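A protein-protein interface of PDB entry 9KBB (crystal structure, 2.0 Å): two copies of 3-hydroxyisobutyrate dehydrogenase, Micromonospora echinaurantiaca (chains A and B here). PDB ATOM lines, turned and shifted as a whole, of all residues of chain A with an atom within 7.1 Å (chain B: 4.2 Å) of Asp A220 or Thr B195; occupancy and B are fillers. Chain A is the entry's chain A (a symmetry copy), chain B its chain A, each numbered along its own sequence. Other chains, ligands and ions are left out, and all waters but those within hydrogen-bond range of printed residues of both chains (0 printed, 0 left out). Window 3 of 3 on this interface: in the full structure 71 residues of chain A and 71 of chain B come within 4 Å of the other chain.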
ATOM      1  N   PRO A 213      -0.980 -15.179 -19.155  1.00  0.00           N
ATOM      2  CA  PRO A 213      -0.382 -15.166 -20.505  1.00  0.00           C
ATOM      3  C   PRO A 213       0.028 -16.538 -21.008  1.00  0.00           C
ATOM      4  O   PRO A 213      -0.174 -16.839 -22.191  1.00  0.00           O
ATOM      5  CB  PRO A 213       0.829 -14.234 -20.338  1.00  0.00           C
ATOM      6  CG  PRO A 213       0.455 -13.343 -19.218  1.00  0.00           C
ATOM      7  CD  PRO A 213      -0.310 -14.214 -18.265  1.00  0.00           C
ATOM      8  N   ALA A 214       0.609 -17.377 -20.148  1.00  0.00           N
ATOM      9  CA  ALA A 214       0.999 -18.710 -20.592  1.00  0.00           C
ATOM     10  C   ALA A 214      -0.227 -19.550 -20.922  1.00  0.00           C
ATOM     11  O   ALA A 214      -0.227 -20.300 -21.904  1.00  0.00           O
ATOM     12  CB  ALA A 214       1.846 -19.396 -19.520  1.00  0.00           C
ATOM     13  N   LEU A 215      -1.283 -19.426 -20.116  1.00  0.00           N
ATOM     14  CA  LEU A 215      -2.530 -20.129 -20.397  1.00  0.00           C
ATOM     15  C   LEU A 215      -3.079 -19.730 -21.761  1.00  0.00           C
ATOM     16  O   LEU A 215      -3.459 -20.589 -22.569  1.00  0.00           O
ATOM     17  CB  LEU A 215      -3.550 -19.832 -19.296  1.00  0.00           C
ATOM     18  CG  LEU A 215      -3.465 -20.617 -17.988  1.00  0.00           C
ATOM     19  CD1 LEU A 215      -4.639 -20.266 -17.093  1.00  0.00           C
ATOM     20  CD2 LEU A 215      -3.425 -22.114 -18.253  1.00  0.00           C
ATOM     21  N   ALA A 216      -3.117 -18.422 -22.034  1.00  0.00           N
ATOM     22  CA  ALA A 216      -3.628 -17.938 -23.313  1.00  0.00           C
ATOM     23  C   ALA A 216      -2.763 -18.422 -24.470  1.00  0.00           C
ATOM     24  O   ALA A 216      -3.281 -18.766 -25.541  1.00  0.00           O
ATOM     25  CB  ALA A 216      -3.701 -16.413 -23.296  1.00  0.00           C
ATOM     26  N   ARG A 217      -1.442 -18.460 -24.269  1.00  0.00           N
ATOM     27  CA  ARG A 217      -0.545 -18.967 -25.303  1.00  0.00           C
ATOM     28  C   ARG A 217      -0.847 -20.427 -25.620  1.00  0.00           C
ATOM     29  O   ARG A 217      -0.861 -20.827 -26.788  1.00  0.00           O
ATOM     30  CB  ARG A 217       0.910 -18.804 -24.861  1.00  0.00           C
ATOM     31  CG  ARG A 217       1.495 -17.443 -25.197  1.00  0.00           C
ATOM     32  CD  ARG A 217       3.009 -17.423 -25.075  1.00  0.00           C
ATOM     33  NE  ARG A 217       3.443 -17.650 -23.705  1.00  0.00           N
ATOM     34  CZ  ARG A 217       3.613 -16.695 -22.800  1.00  0.00           C
ATOM     35  NH1 ARG A 217       3.343 -15.429 -23.073  1.00  0.00           N
ATOM     36  NH2 ARG A 217       4.063 -17.020 -21.592  1.00  0.00           N
ATOM     37  N   GLY A 218      -1.098 -21.232 -24.588  1.00  0.00           N
ATOM     38  CA  GLY A 218      -1.412 -22.633 -24.822  1.00  0.00           C
ATOM     39  C   GLY A 218      -2.723 -22.821 -25.536  1.00  0.00           C
ATOM     40  O   GLY A 218      -2.851 -23.689 -26.412  1.00  0.00           O
ATOM     41  N   VAL A 219      -3.740 -22.021 -25.190  1.00  0.00           N
ATOM     42  CA  VAL A 219      -5.038 -22.111 -25.841  1.00  0.00           C
ATOM     43  C   VAL A 219      -4.907 -21.815 -27.333  1.00  0.00           C
ATOM     44  O   VAL A 219      -5.389 -22.569 -28.181  1.00  0.00           O
ATOM     45  CB  VAL A 219      -6.048 -21.159 -25.179  1.00  0.00           C
ATOM     46  CG1 VAL A 219      -7.320 -21.077 -26.002  1.00  0.00           C
ATOM     47  CG2 VAL A 219      -6.355 -21.605 -23.760  1.00  0.00           C
ATOM     48  N   ASP A 220      -4.264 -20.695 -27.662  1.00  0.00           N
ATOM     49  CA  ASP A 220      -4.131 -20.319 -29.065  1.00  0.00           C
ATOM     50  C   ASP A 220      -3.221 -21.283 -29.815  1.00  0.00           C
ATOM     51  O   ASP A 220      -3.475 -21.594 -30.985  1.00  0.00           O
ATOM     52  CB  ASP A 220      -3.612 -18.887 -29.177  1.00  0.00           C
ATOM     53  CG  ASP A 220      -4.602 -17.868 -28.650  1.00  0.00           C
ATOM     54  OD1 ASP A 220      -5.788 -18.221 -28.481  1.00  0.00           O
ATOM     55  OD2 ASP A 220      -4.191 -16.716 -28.401  1.00  0.00           O
ATOM     56  N   SER A 221      -2.166 -21.773 -29.162  1.00  0.00           N
ATOM     57  CA  SER A 221      -1.206 -22.621 -29.857  1.00  0.00           C
ATOM     58  C   SER A 221      -1.681 -24.064 -29.954  1.00  0.00           C
ATOM     59  O   SER A 221      -1.274 -24.787 -30.870  1.00  0.00           O
ATOM     60  CB  SER A 221       0.148 -22.587 -29.150  1.00  0.00           C
ATOM     61  OG  SER A 221       0.101 -23.323 -27.939  1.00  0.00           O
ATOM     62  N   GLY A 222      -2.534 -24.504 -29.030  1.00  0.00           N
ATOM     63  CA  GLY A 222      -2.823 -25.914 -28.900  1.00  0.00           C
ATOM     64  C   GLY A 222      -1.730 -26.705 -28.218  1.00  0.00           C
ATOM     65  O   GLY A 222      -1.874 -27.923 -28.064  1.00  0.00           O
ATOM     66  N   ASP A 223      -0.640 -26.055 -27.810  1.00  0.00           N
ATOM     67  CA  ASP A 223       0.441 -26.702 -27.066  1.00  0.00           C
ATOM     68  C   ASP A 223       0.193 -26.474 -25.580  1.00  0.00           C
ATOM     69  O   ASP A 223       0.573 -25.440 -25.032  1.00  0.00           O
ATOM     70  CB  ASP A 223       1.799 -26.151 -27.496  1.00  0.00           C
ATOM     71  CG  ASP A 223       2.972 -26.934 -26.913  1.00  0.00           C
ATOM     72  OD1 ASP A 223       2.795 -27.639 -25.900  1.00  0.00           O
ATOM     73  OD2 ASP A 223       4.088 -26.834 -27.460  1.00  0.00           O
ATOM     74  N   HIS A 224      -0.423 -27.451 -24.924  1.00  0.00           N
ATOM     75  CA  HIS A 224      -0.788 -27.319 -23.515  1.00  0.00           C
ATOM     76  C   HIS A 224       0.352 -27.743 -22.599  1.00  0.00           C
ATOM     77  O   HIS A 224       0.221 -28.616 -21.745  1.00  0.00           O
ATOM     78  CB  HIS A 224      -2.057 -28.112 -23.240  1.00  0.00           C
ATOM     79  CG  HIS A 224      -3.168 -27.778 -24.184  1.00  0.00           C
ATOM     80  ND1 HIS A 224      -3.645 -26.494 -24.343  1.00  0.00           N
ATOM     81  CD2 HIS A 224      -3.865 -28.550 -25.050  1.00  0.00           C
ATOM     82  CE1 HIS A 224      -4.605 -26.494 -25.253  1.00  0.00           C
ATOM     83  NE2 HIS A 224      -4.756 -27.728 -25.696  1.00  0.00           N
ATOM     84  N   SER A 276      -4.559 -24.955 -19.782  1.00  0.00           N
ATOM     85  CA  SER A 276      -5.011 -24.525 -21.102  1.00  0.00           C
ATOM     86  C   SER A 276      -5.740 -25.647 -21.833  1.00  0.00           C
ATOM     87  O   SER A 276      -6.539 -25.381 -22.739  1.00  0.00           O
ATOM     88  CB  SER A 276      -3.822 -24.041 -21.931  1.00  0.00           C
ATOM     89  OG  SER A 276      -2.936 -25.108 -22.215  1.00  0.00           O
ATOM     90  N   PRO B 193      -8.620 -14.499 -30.502  1.00  0.00           N
ATOM     91  CA  PRO B 193      -7.529 -15.187 -29.796  1.00  0.00           C
ATOM     92  C   PRO B 193      -7.498 -14.826 -28.318  1.00  0.00           C
ATOM     93  O   PRO B 193      -7.852 -13.714 -27.918  1.00  0.00           O
ATOM     94  CB  PRO B 193      -6.267 -14.697 -30.521  1.00  0.00           C
ATOM     95  CG  PRO B 193      -6.755 -14.029 -31.784  1.00  0.00           C
ATOM     96  CD  PRO B 193      -8.107 -13.486 -31.436  1.00  0.00           C
ATOM     97  N   ALA B 194      -7.066 -15.796 -27.506  1.00  0.00           N
ATOM     98  CA  ALA B 194      -6.978 -15.571 -26.070  1.00  0.00           C
ATOM     99  C   ALA B 194      -5.856 -14.600 -25.724  1.00  0.00           C
ATOM    100  O   ALA B 194      -5.941 -13.894 -24.713  1.00  0.00           O
ATOM    101  CB  ALA B 194      -6.776 -16.899 -25.343  1.00  0.00           C
ATOM    102  N   THR B 195      -4.813 -14.537 -26.556  1.00  0.00           N
ATOM    103  CA  THR B 195      -3.648 -13.723 -26.218  1.00  0.00           C
ATOM    104  C   THR B 195      -4.002 -12.244 -26.148  1.00  0.00           C
ATOM    105  O   THR B 195      -3.531 -11.531 -25.257  1.00  0.00           O
ATOM    106  CB  THR B 195      -2.523 -13.958 -27.230  1.00  0.00           C
ATOM    107  OG1 THR B 195      -2.075 -15.314 -27.131  1.00  0.00           O
ATOM    108  CG2 THR B 195      -1.346 -13.034 -26.953  1.00  0.00           C
ATOM    109  N   GLY B 196      -4.827 -11.762 -27.082  1.00  0.00           N
ATOM    110  CA  GLY B 196      -5.211 -10.360 -27.072  1.00  0.00           C
ATOM    111  C   GLY B 196      -6.231 -10.005 -26.018  1.00  0.00           C
ATOM    112  O   GLY B 196      -6.352  -8.827 -25.656  1.00  0.00           O
ATOM    113  N   PHE B 197      -6.971 -11.002 -25.527  1.00  0.00           N
ATOM    114  CA  PHE B 197      -7.955 -10.792 -24.474  1.00  0.00           C
ATOM    115  C   PHE B 197      -7.316 -10.639 -23.101  1.00  0.00           C
ATOM    116  O   PHE B 197      -7.900  -9.998 -22.224  1.00  0.00           O
ATOM    117  CB  PHE B 197      -8.926 -11.971 -24.466  1.00  0.00           C
ATOM    118  CG  PHE B 197      -9.933 -11.950 -23.358  1.00  0.00           C
ATOM    119  CD1 PHE B 197     -10.918 -10.982 -23.312  1.00  0.00           C
ATOM    120  CD2 PHE B 197      -9.894 -12.912 -22.362  1.00  0.00           C
ATOM    121  CE1 PHE B 197     -11.856 -10.972 -22.287  1.00  0.00           C
ATOM    122  CE2 PHE B 197     -10.824 -12.905 -21.334  1.00  0.00           C
ATOM    123  CZ  PHE B 197     -11.804 -11.936 -21.297  1.00  0.00           C
ATOM    124  N   THR B 198      -6.116 -11.183 -22.911  1.00  0.00           N
ATOM    125  CA  THR B 198      -5.509 -11.232 -21.584  1.00  0.00           C
ATOM    126  C   THR B 198      -5.310  -9.854 -20.952  1.00  0.00           C
ATOM    127  O   THR B 198      -5.640  -9.701 -19.768  1.00  0.00           O
ATOM    128  CB  THR B 198      -4.193 -12.015 -21.657  1.00  0.00           C
ATOM    129  OG1 THR B 198      -4.496 -13.402 -21.821  1.00  0.00           O
ATOM    130  CG2 THR B 198      -3.375 -11.833 -20.381  1.00  0.00           C
ATOM    131  N   PRO B 199      -4.778  -8.836 -21.647  1.00  0.00           N
ATOM    132  CA  PRO B 199      -4.681  -7.508 -21.002  1.00  0.00           C
ATOM    133  C   PRO B 199      -6.003  -6.976 -20.461  1.00  0.00           C
ATOM    134  O   PRO B 199      -6.051  -6.486 -19.325  1.00  0.00           O
ATOM    135  CB  PRO B 199      -4.137  -6.628 -22.133  1.00  0.00           C
ATOM    136  CG  PRO B 199      -3.324  -7.557 -22.949  1.00  0.00           C
ATOM    137  CD  PRO B 199      -4.119  -8.834 -22.967  1.00  0.00           C
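OD1 of Asp A220 sits at hydrogen-bond distance from N of Ala B194 (2.9 Å).
The side-chain hydroxyl of Thr B195 sits at hydrogen-bond distance from the side-chain carboxylate of Asp A220 (2.8 Å).
The side-chain hydroxyl (OG1) of Thr B198 sits at hydrogen-bond distance from the backbone carbonyl oxygen (O) of Ala B194.
CB of Ala A216 touches O of Ala B194, 3.7 Å away.
CB of Ala A216 touches N of Thr B195, 3.9 Å away.
Thr B198 touches Ala A216.
Pro B193 touches Asp A220 (CB to OD2, 3.6 Å).
Asp A220 touches just these residues of chain B: Pro B193, Ala B194 and Thr B195.
Thr B195 touches just these residues of chain A: Ala A216 and Asp A220.
Printed residues of chain B within 4 Å of Ala A216: Ala B194 (3.7 Å), Thr B195 (3.9 Å) and Thr B198 (3.4 Å).
Printed residues of chain A within 4 Å of Thr B198: Ala A216 (3.4 Å).
Of the printed residues of chain A, Pro B193 touches Asp A220 (3.6 Å).
Of the printed residues of chain A, Ala B194 touches Ala A216 and Asp A220.
Leu A215 touches none of the printed residues of chain B.
Val A219 touches none of the printed residues of chain B.
The nearest printed residue of chain B that does not touch Asp A220 is Gly B196 (5.2 Å).
The nearest residue of chain A that does not touch Thr B195 is Arg A217 (4.3 Å).
Of the 7 printed residues of chain B, 4 touch a printed residue of chain A.
Printed residues of chain B that touch a printed residue of chain A: Pro B193, Ala B194, Thr B195 and Thr B198.
Hydrophobic or aromatic side chains of chain B that line the printed part of chain A: Pro B193 and Ala B194.
Of the 13 printed residues of chain A, 2 touch a printed residue of chain B.
Printed residues of chain A that touch a printed residue of chain B: Ala A216 and Asp A220.
Hydrophobic or aromatic side chains of chain A that line the printed part of chain B: Ala A216.
Among the printed residues, no Asp or Glu carboxylate lies within 4 Å of a Lys or Arg side-chain nitrogen of the other chain.
No position is printed for both chains.
Of the 6 pairs that touch across the chains among the printed residues, none has its exchanged pair printed and touching as well.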
